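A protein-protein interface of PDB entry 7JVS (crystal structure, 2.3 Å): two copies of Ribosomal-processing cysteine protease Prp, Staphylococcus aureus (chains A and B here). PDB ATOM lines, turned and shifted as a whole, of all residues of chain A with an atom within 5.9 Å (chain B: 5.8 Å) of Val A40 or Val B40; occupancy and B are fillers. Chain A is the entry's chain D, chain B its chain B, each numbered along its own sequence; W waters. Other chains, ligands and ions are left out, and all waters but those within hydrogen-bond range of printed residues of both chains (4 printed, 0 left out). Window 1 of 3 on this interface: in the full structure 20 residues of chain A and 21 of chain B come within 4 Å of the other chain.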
ATOM      1  N   ALA A  35     -16.945   4.105  -1.041  1.00  0.00           N
ATOM      2  CA  ALA A  35     -18.031   5.089  -0.981  1.00  0.00           C
ATOM      3  C   ALA A  35     -18.307   5.725  -2.357  1.00  0.00           C
ATOM      4  O   ALA A  35     -19.450   5.922  -2.726  1.00  0.00           O
ATOM      5  CB  ALA A  35     -17.704   6.178   0.042  1.00  0.00           C
ATOM      6  N   GLY A  36     -17.238   6.040  -3.097  1.00  0.00           N
ATOM      7  CA  GLY A  36     -17.293   6.563  -4.452  1.00  0.00           C
ATOM      8  C   GLY A  36     -17.970   5.617  -5.428  1.00  0.00           C
ATOM      9  O   GLY A  36     -18.924   5.999  -6.096  1.00  0.00           O
ATOM     10  N   ALA A  37     -17.475   4.382  -5.503  1.00  0.00           N
ATOM     11  CA  ALA A  37     -18.001   3.362  -6.432  1.00  0.00           C
ATOM     12  C   ALA A  37     -19.437   3.002  -6.109  1.00  0.00           C
ATOM     13  O   ALA A  37     -20.246   2.826  -7.008  1.00  0.00           O
ATOM     14  CB  ALA A  37     -17.138   2.104  -6.383  1.00  0.00           C
ATOM     15  N   SER A  38     -19.748   2.886  -4.812  1.00  0.00           N
ATOM     16  CA  SER A  38     -21.101   2.467  -4.470  1.00  0.00           C
ATOM     17  C   SER A  38     -22.094   3.608  -4.759  1.00  0.00           C
ATOM     18  O   SER A  38     -23.104   3.409  -5.393  1.00  0.00           O
ATOM     19  CB  SER A  38     -21.179   2.009  -3.012  1.00  0.00           C
ATOM     20  OG  SER A  38     -20.586   0.716  -2.873  1.00  0.00           O
ATOM     21  N   ALA A  39     -21.773   4.870  -4.468  1.00  0.00           N
ATOM     22  CA  ALA A  39     -22.676   5.973  -4.777  1.00  0.00           C
ATOM     23  C   ALA A  39     -22.950   6.060  -6.293  1.00  0.00           C
ATOM     24  O   ALA A  39     -24.038   6.397  -6.705  1.00  0.00           O
ATOM     25  CB  ALA A  39     -22.094   7.279  -4.253  1.00  0.00           C
ATOM     26  N   VAL A  40     -21.921   5.774  -7.103  1.00  0.00           N
ATOM     27  CA  VAL A  40     -22.026   5.761  -8.555  1.00  0.00           C
ATOM     28  C   VAL A  40     -22.914   4.583  -9.039  1.00  0.00           C
ATOM     29  O   VAL A  40     -23.780   4.753  -9.896  1.00  0.00           O
ATOM     30  CB  VAL A  40     -20.617   5.695  -9.197  1.00  0.00           C
ATOM     31  CG1 VAL A  40     -20.659   5.282 -10.657  1.00  0.00           C
ATOM     32  CG2 VAL A  40     -19.894   7.033  -9.036  1.00  0.00           C
ATOM     33  N   LEU A  41     -22.694   3.400  -8.466  1.00  0.00           N
ATOM     34  CA  LEU A  41     -23.474   2.234  -8.861  1.00  0.00           C
ATOM     35  C   LEU A  41     -24.945   2.337  -8.474  1.00  0.00           C
ATOM     36  O   LEU A  41     -25.825   2.292  -9.330  1.00  0.00           O
ATOM     37  CB  LEU A  41     -22.898   0.956  -8.272  1.00  0.00           C
ATOM     38  CG  LEU A  41     -23.420  -0.273  -9.030  1.00  0.00           C
ATOM     39  CD1 LEU A  41     -22.243  -1.182  -9.350  1.00  0.00           C
ATOM     40  CD2 LEU A  41     -24.508  -1.036  -8.284  1.00  0.00           C
ATOM     41  N   PHE A  42     -25.245   2.571  -7.193  1.00  0.00           N
ATOM     42  CA  PHE A  42     -26.627   2.613  -6.735  1.00  0.00           C
ATOM     43  C   PHE A  42     -27.340   3.814  -7.311  1.00  0.00           C
ATOM     44  O   PHE A  42     -28.532   3.746  -7.626  1.00  0.00           O
ATOM     45  CB  PHE A  42     -26.713   2.591  -5.207  1.00  0.00           C
ATOM     46  CG  PHE A  42     -26.025   1.399  -4.570  1.00  0.00           C
ATOM     47  CD1 PHE A  42     -26.266   0.092  -5.014  1.00  0.00           C
ATOM     48  CD2 PHE A  42     -25.111   1.586  -3.545  1.00  0.00           C
ATOM     49  CE1 PHE A  42     -25.608  -0.997  -4.432  1.00  0.00           C
ATOM     50  CE2 PHE A  42     -24.467   0.501  -2.941  1.00  0.00           C
ATOM     51  CZ  PHE A  42     -24.704  -0.789  -3.393  1.00  0.00           C
ATOM     52  N   GLY A  43     -26.593   4.895  -7.531  1.00  0.00           N
ATOM     53  CA  GLY A  43     -27.086   6.083  -8.185  1.00  0.00           C
ATOM     54  C   GLY A  43     -27.555   5.781  -9.602  1.00  0.00           C
ATOM     55  O   GLY A  43     -28.638   6.188  -9.998  1.00  0.00           O
ATOM     56  N   SER A  44     -26.730   5.045 -10.347  1.00  0.00           N
ATOM     57  CA  SER A  44     -27.014   4.661 -11.722  1.00  0.00           C
ATOM     58  C   SER A  44     -28.259   3.790 -11.821  1.00  0.00           C
ATOM     59  O   SER A  44     -29.102   4.018 -12.658  1.00  0.00           O
ATOM     60  CB  SER A  44     -25.823   3.904 -12.318  1.00  0.00           C
ATOM     61  OG  SER A  44     -24.689   4.734 -12.305  1.00  0.00           O
ATOM     62  N   VAL A  45     -28.358   2.786 -10.952  1.00  0.00           N
ATOM     63  CA  VAL A  45     -29.516   1.886 -10.925  1.00  0.00           C
ATOM     64  C   VAL A  45     -30.798   2.674 -10.688  1.00  0.00           C
ATOM     65  O   VAL A  45     -31.776   2.467 -11.384  1.00  0.00           O
ATOM     66  CB  VAL A  45     -29.362   0.798  -9.844  1.00  0.00           C
ATOM     67  CG1 VAL A  45     -30.667   0.013  -9.663  1.00  0.00           C
ATOM     68  CG2 VAL A  45     -28.203  -0.112 -10.210  1.00  0.00           C
ATOM     69  N   THR A  85     -22.172   5.509 -18.794  1.00  0.00           N
ATOM     70  CA  THR A  85     -21.802   6.653 -17.974  1.00  0.00           C
ATOM     71  C   THR A  85     -21.214   6.161 -16.660  1.00  0.00           C
ATOM     72  O   THR A  85     -20.266   6.742 -16.132  1.00  0.00           O
ATOM     73  CB  THR A  85     -23.019   7.549 -17.678  1.00  0.00           C
ATOM     74  OG1 THR A  85     -23.494   8.136 -18.895  1.00  0.00           O
ATOM     75  CG2 THR A  85     -22.646   8.649 -16.697  1.00  0.00           C
ATOM     76  N   MET A  86     -21.799   5.091 -16.130  1.00  0.00           N
ATOM     77  CA  MET A  86     -21.341   4.503 -14.879  1.00  0.00           C
ATOM     78  C   MET A  86     -19.927   3.970 -15.059  1.00  0.00           C
ATOM     79  O   MET A  86     -19.058   4.182 -14.214  1.00  0.00           O
ATOM     80  CB  MET A  86     -22.274   3.370 -14.452  1.00  0.00           C
ATOM     81  CG  MET A  86     -21.990   2.823 -13.064  1.00  0.00           C
ATOM     82  SD  MET A  86     -23.071   1.446 -12.627  1.00  0.00           S
ATOM     83  CE  MET A  86     -22.484   0.187 -13.757  1.00  0.00           C
ATOM     84  N   SER A  89     -17.441   6.744 -15.075  1.00  0.00           N
ATOM     85  CA  SER A  89     -17.269   7.253 -13.721  1.00  0.00           C
ATOM     86  C   SER A  89     -16.414   6.290 -12.909  1.00  0.00           C
ATOM     87  O   SER A  89     -15.591   6.708 -12.095  1.00  0.00           O
ATOM     88  CB  SER A  89     -18.628   7.447 -13.046  1.00  0.00           C
ATOM     89  OG  SER A  89     -19.508   8.180 -13.880  1.00  0.00           O
ATOM     90  N   LEU A  90     -16.597   5.012 -13.121  1.00  0.00           N
ATOM     91  CA  LEU A  90     -15.836   3.984 -12.423  1.00  0.00           C
ATOM     92  C   LEU A  90     -14.391   3.995 -12.906  1.00  0.00           C
ATOM     93  O   LEU A  90     -13.466   3.739 -12.135  1.00  0.00           O
ATOM     94  CB  LEU A  90     -16.464   2.610 -12.651  1.00  0.00           C
ATOM     95  CG  LEU A  90     -17.768   2.363 -11.892  1.00  0.00           C
ATOM     96  CD1 LEU A  90     -18.162   0.898 -11.957  1.00  0.00           C
ATOM     97  CD2 LEU A  90     -17.644   2.823 -10.449  1.00  0.00           C
ATOM     98  N   ILE A  93     -12.369   6.759 -11.306  1.00  0.00           N
ATOM     99  CA  ILE A  93     -11.898   6.357  -9.986  1.00  0.00           C
ATOM    100  C   ILE A  93     -10.653   5.460 -10.117  1.00  0.00           C
ATOM    101  O   ILE A  93      -9.658   5.691  -9.449  1.00  0.00           O
ATOM    102  CB  ILE A  93     -12.993   5.678  -9.128  1.00  0.00           C
ATOM    103  CG1 ILE A  93     -14.209   6.592  -8.955  1.00  0.00           C
ATOM    104  CG2 ILE A  93     -12.437   5.331  -7.749  1.00  0.00           C
ATOM    105  CD1 ILE A  93     -15.441   5.920  -8.347  1.00  0.00           C
ATOM    106  N   ALA B  35     -16.653  11.794  -0.916  1.00  0.00           N
ATOM    107  CA  ALA B  35     -16.217  10.772  -1.878  1.00  0.00           C
ATOM    108  C   ALA B  35     -17.361  10.378  -2.835  1.00  0.00           C
ATOM    109  O   ALA B  35     -17.139  10.258  -4.035  1.00  0.00           O
ATOM    110  CB  ALA B  35     -15.681   9.558  -1.158  1.00  0.00           C
ATOM    111  N   GLY B  36     -18.572  10.211  -2.281  1.00  0.00           N
ATOM    112  CA  GLY B  36     -19.773   9.921  -3.047  1.00  0.00           C
ATOM    113  C   GLY B  36     -20.110  11.016  -4.076  1.00  0.00           C
ATOM    114  O   GLY B  36     -20.243  10.741  -5.278  1.00  0.00           O
ATOM    115  N   ALA B  37     -20.246  12.259  -3.596  1.00  0.00           N
ATOM    116  CA  ALA B  37     -20.653  13.378  -4.454  1.00  0.00           C
ATOM    117  C   ALA B  37     -19.604  13.692  -5.512  1.00  0.00           C
ATOM    118  O   ALA B  37     -19.955  13.957  -6.669  1.00  0.00           O
ATOM    119  CB  ALA B  37     -20.977  14.601  -3.641  1.00  0.00           C
ATOM    120  N   SER B  38     -18.326  13.612  -5.118  1.00  0.00           N
ATOM    121  CA  SER B  38     -17.219  13.884  -6.021  1.00  0.00           C
ATOM    122  C   SER B  38     -17.180  12.877  -7.161  1.00  0.00           C
ATOM    123  O   SER B  38     -17.124  13.272  -8.336  1.00  0.00           O
ATOM    124  CB  SER B  38     -15.881  13.901  -5.256  1.00  0.00           C
ATOM    125  OG  SER B  38     -15.883  14.920  -4.247  1.00  0.00           O
ATOM    126  N   ALA B  39     -17.233  11.581  -6.818  1.00  0.00           N
ATOM    127  CA  ALA B  39     -17.187  10.509  -7.817  1.00  0.00           C
ATOM    128  C   ALA B  39     -18.312  10.655  -8.843  1.00  0.00           C
ATOM    129  O   ALA B  39     -18.110  10.425 -10.038  1.00  0.00           O
ATOM    130  CB  ALA B  39     -17.250   9.142  -7.171  1.00  0.00           C
ATOM    131  N   VAL B  40     -19.485  11.060  -8.361  1.00  0.00           N
ATOM    132  CA  VAL B  40     -20.664  11.227  -9.196  1.00  0.00           C
ATOM    133  C   VAL B  40     -20.526  12.445 -10.109  1.00  0.00           C
ATOM    134  O   VAL B  40     -20.803  12.361 -11.306  1.00  0.00           O
ATOM    135  CB  VAL B  40     -21.932  11.295  -8.320  1.00  0.00           C
ATOM    136  CG1 VAL B  40     -23.118  11.786  -9.122  1.00  0.00           C
ATOM    137  CG2 VAL B  40     -22.206   9.916  -7.736  1.00  0.00           C
ATOM    138  N   LEU B  41     -20.069  13.566  -9.535  1.00  0.00           N
ATOM    139  CA  LEU B  41     -19.841  14.796 -10.287  1.00  0.00           C
ATOM    140  C   LEU B  41     -18.833  14.621 -11.413  1.00  0.00           C
ATOM    141  O   LEU B  41     -19.177  14.801 -12.583  1.00  0.00           O
ATOM    142  CB  LEU B  41     -19.390  15.923  -9.365  1.00  0.00           C
ATOM    143  CG  LEU B  41     -19.154  17.263 -10.039  1.00  0.00           C
ATOM    144  CD1 LEU B  41     -20.407  17.653 -10.845  1.00  0.00           C
ATOM    145  CD2 LEU B  41     -18.724  18.328  -9.028  1.00  0.00           C
ATOM    146  N   PHE B  42     -17.594  14.287 -11.043  1.00  0.00           N
ATOM    147  CA  PHE B  42     -16.492  14.243 -11.998  1.00  0.00           C
ATOM    148  C   PHE B  42     -16.702  13.134 -12.995  1.00  0.00           C
ATOM    149  O   PHE B  42     -16.337  13.258 -14.167  1.00  0.00           O
ATOM    150  CB  PHE B  42     -15.159  14.096 -11.268  1.00  0.00           C
ATOM    151  CG  PHE B  42     -14.806  15.311 -10.433  1.00  0.00           C
ATOM    152  CD1 PHE B  42     -14.826  15.227  -9.052  1.00  0.00           C
ATOM    153  CD2 PHE B  42     -14.465  16.526 -11.016  1.00  0.00           C
ATOM    154  CE1 PHE B  42     -14.500  16.332  -8.263  1.00  0.00           C
ATOM    155  CE2 PHE B  42     -14.119  17.615 -10.243  1.00  0.00           C
ATOM    156  CZ  PHE B  42     -14.142  17.520  -8.855  1.00  0.00           C
ATOM    157  N   GLY B  43     -17.335  12.049 -12.529  1.00  0.00           N
ATOM    158  CA  GLY B  43     -17.708  10.932 -13.367  1.00  0.00           C
ATOM    159  C   GLY B  43     -18.657  11.370 -14.462  1.00  0.00           C
ATOM    160  O   GLY B  43     -18.462  11.037 -15.621  1.00  0.00           O
ATOM    161  N   SER B  44     -19.690  12.116 -14.083  1.00  0.00           N
ATOM    162  CA  SER B  44     -20.689  12.592 -15.035  1.00  0.00           C
ATOM    163  C   SER B  44     -20.106  13.577 -16.043  1.00  0.00           C
ATOM    164  O   SER B  44     -20.296  13.425 -17.250  1.00  0.00           O
ATOM    165  CB  SER B  44     -21.851  13.251 -14.289  1.00  0.00           C
ATOM    166  OG  SER B  44     -22.547  12.309 -13.493  1.00  0.00           O
ATOM    167  N   VAL B  45     -19.402  14.587 -15.543  1.00  0.00           N
ATOM    168  CA  VAL B  45     -18.805  15.602 -16.404  1.00  0.00           C
ATOM    169  C   VAL B  45     -17.902  14.978 -17.465  1.00  0.00           C
ATOM    170  O   VAL B  45     -18.011  15.298 -18.648  1.00  0.00           O
ATOM    171  CB  VAL B  45     -17.994  16.624 -15.586  1.00  0.00           C
ATOM    172  CG1 VAL B  45     -17.155  17.498 -16.506  1.00  0.00           C
ATOM    173  CG2 VAL B  45     -18.924  17.477 -14.737  1.00  0.00           C
ATOM    174  N   THR B  85     -29.296  11.784 -14.544  1.00  0.00           N
ATOM    175  CA  THR B  85     -28.690  10.682 -13.822  1.00  0.00           C
ATOM    176  C   THR B  85     -27.894  11.216 -12.627  1.00  0.00           C
ATOM    177  O   THR B  85     -28.109  10.789 -11.487  1.00  0.00           O
ATOM    178  CB  THR B  85     -27.843   9.839 -14.777  1.00  0.00           C
ATOM    179  OG1 THR B  85     -28.707   9.269 -15.784  1.00  0.00           O
ATOM    180  CG2 THR B  85     -27.108   8.716 -14.052  1.00  0.00           C
ATOM    181  N   MET B  86     -27.023  12.198 -12.882  1.00  0.00           N
ATOM    182  CA  MET B  86     -26.247  12.835 -11.833  1.00  0.00           C
ATOM    183  C   MET B  86     -27.156  13.303 -10.692  1.00  0.00           C
ATOM    184  O   MET B  86     -26.875  13.037  -9.521  1.00  0.00           O
ATOM    185  CB  MET B  86     -25.451  14.017 -12.389  1.00  0.00           C
ATOM    186  CG  MET B  86     -24.510  14.639 -11.378  1.00  0.00           C
ATOM    187  SD  MET B  86     -23.536  15.965 -12.107  1.00  0.00           S
ATOM    188  CE  MET B  86     -24.691  17.311 -11.857  1.00  0.00           C
ATOM    189  N   SER B  89     -28.556  10.444  -8.620  1.00  0.00           N
ATOM    190  CA  SER B  89     -27.489   9.887  -7.799  1.00  0.00           C
ATOM    191  C   SER B  89     -27.249  10.761  -6.570  1.00  0.00           C
ATOM    192  O   SER B  89     -27.135  10.247  -5.449  1.00  0.00           O
ATOM    193  CB  SER B  89     -26.188   9.736  -8.594  1.00  0.00           C
ATOM    194  OG  SER B  89     -26.264   8.664  -9.514  1.00  0.00           O
ATOM    195  N   LEU B  90     -27.192  12.081  -6.779  1.00  0.00           N
ATOM    196  CA  LEU B  90     -26.946  12.984  -5.655  1.00  0.00           C
ATOM    197  C   LEU B  90     -28.137  13.025  -4.697  1.00  0.00           C
ATOM    198  O   LEU B  90     -27.952  13.137  -3.481  1.00  0.00           O
ATOM    199  CB  LEU B  90     -26.571  14.393  -6.116  1.00  0.00           C
ATOM    200  CG  LEU B  90     -25.326  14.484  -7.006  1.00  0.00           C
ATOM    201  CD1 LEU B  90     -25.272  15.818  -7.739  1.00  0.00           C
ATOM    202  CD2 LEU B  90     -24.049  14.286  -6.208  1.00  0.00           C
ATOM    203  N   ILE B  93     -27.809  10.169  -2.335  1.00  0.00           N
ATOM    204  CA  ILE B  93     -26.913  10.512  -1.232  1.00  0.00           C
ATOM    205  C   ILE B  93     -27.631  11.425  -0.218  1.00  0.00           C
ATOM    206  O   ILE B  93     -27.541  11.192   0.976  1.00  0.00           O
ATOM    207  CB  ILE B  93     -25.592  11.144  -1.727  1.00  0.00           C
ATOM    208  CG1 ILE B  93     -24.853  10.197  -2.676  1.00  0.00           C
ATOM    209  CG2 ILE B  93     -24.676  11.459  -0.551  1.00  0.00           C
ATOM    210  CD1 ILE B  93     -23.732  10.858  -3.454  1.00  0.00           C
HETATM  211  O   HOH W   1     -24.217   7.709 -10.720  1.00  0.00           O
HETATM  212  O   HOH W   2     -21.296   9.590 -12.189  1.00  0.00           O
HETATM  213  O   HOH W   3     -15.789   9.261 -10.901  1.00  0.00           O
HETATM  214  O   HOH W   4     -25.685   7.453  -5.106  1.00  0.00           O
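Water W4 bridges the backbone carbonyl oxygen (O) of Ala A39 (2.5 Å) and the backbone carbonyl oxygen (O) of Ser B89 (3.2 Å). Water W1 lies within hydrogen-bond range of the side-chain hydroxyl of Ser B89 (2.6 Å), the backbone carbonyl oxygen of Val A40 (3.1 Å) and the side-chain hydroxyl of Ser A44 (3.4 Å). Water W3 lies within hydrogen-bond range of the backbone carbonyl oxygen of Ala B39 and the backbone carbonyl oxygen of Ser A89. Water W2 lies within hydrogen-bond range of OG of Ser A89 (2.8 Å), O of Val B40 (2.9 Å) and OG of Ser B44 (3.3 Å).
Hydrophobic or aromatic side chains of chain A that line the printed part of chain B: Ala A39, Val A40 and Ile A93. Of the 16 printed residues of chain B, 7 touch a printed residue of chain A. Printed residues of chain B that touch a printed residue of chain A: Ala B35, Gly B36, Ala B39, Val B40, Gly B43, Ser B44 and Ser B89. Hydrophobic or aromatic side chains of chain B within 4 Å of the printed part of chain A: Ala B39 and Val B40. Along chain B the printed residues that touch a printed residue of chain A span positions 35 to 89. Among the printed residues, no Asp or Glu carboxylate lies within 4 Å of a Lys or Arg side-chain nitrogen of the other chain.
The side-chain hydroxyl (OG) of Ser B89 sits close to the backbone carbonyl oxygen (O) of Gly A43, 3.5 Å away.
The side-chain hydroxyl (OG) of Ser A44 sits close to the side-chain sulfur (SD) of Met A86 (3.7 Å). The side-chain hydroxyl (OG) of Ser A89 is in hydrogen-bond range of the backbone carbonyl oxygen (O) of Thr A85 (2.8 Å). O of Val B40 is in hydrogen-bond range of OG of Ser B44 (2.8 Å). The side-chain hydroxyl (OG) of Ser A44 is in hydrogen-bond range of the backbone carbonyl oxygen (O) of Val A40 (2.6 Å). The backbone carbonyl oxygen (O) of Thr B85 is in hydrogen-bond range of the side-chain hydroxyl (OG) of Ser B89 (3.4 Å).
CA of Gly A36 touches O of Ala B35 (3.7 Å). Gly A36 touches Ala B39. Ala A39 touches Gly B36 (CB to CA, 3.7 Å). Val A40 touches Ala B39 (CG2 to CB, 3.9 Å). CG2 of Val A40 touches CG2 of Val B40, at 3.9 Å. Ser A44 touches Ser B89 (N to OG, 3.7 Å). CA of Gly B43 touches OG of Ser A89, at 3.3 Å. Ser A89 touches Ser B44. Ile A93 touches Ala B39 (CD1 to CB, 3.9 Å).
Of chain B, only Ala B39 and Val B40 come within 4 Å of Val A40. Val B40 touches one residue of chain A. Printed residues of chain B within 4 Å of Ser A44: Ser B89. Printed residues of chain A within 4 Å of Ala B35: Gly A36 (3.7 Å). The nearest printed residue of chain B that does not touch Val A40 is Ser B89 (4.6 Å). The nearest residue of chain A that does not touch Val B40 is Ala A39 (4.1 Å).
Gly A36 touches Ala B35, but with the chains exchanged Ala A35 does not touch Gly B36 (4.02 Å). Gly A36 touches Ala B39, and with the chains exchanged Ala A39 touches Gly B36. Val A40 touches Ala B39, but with the chains exchanged Ala A39 does not touch Val B40 (4.1 Å). Ser A44 touches Ser B89, and with the chains exchanged Ser A89 touches Ser B44. 16 positions are printed for both chains. Of the 10 pairs that touch across the chains among the printed residues, 7 have their exchanged pair printed and touching as well.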
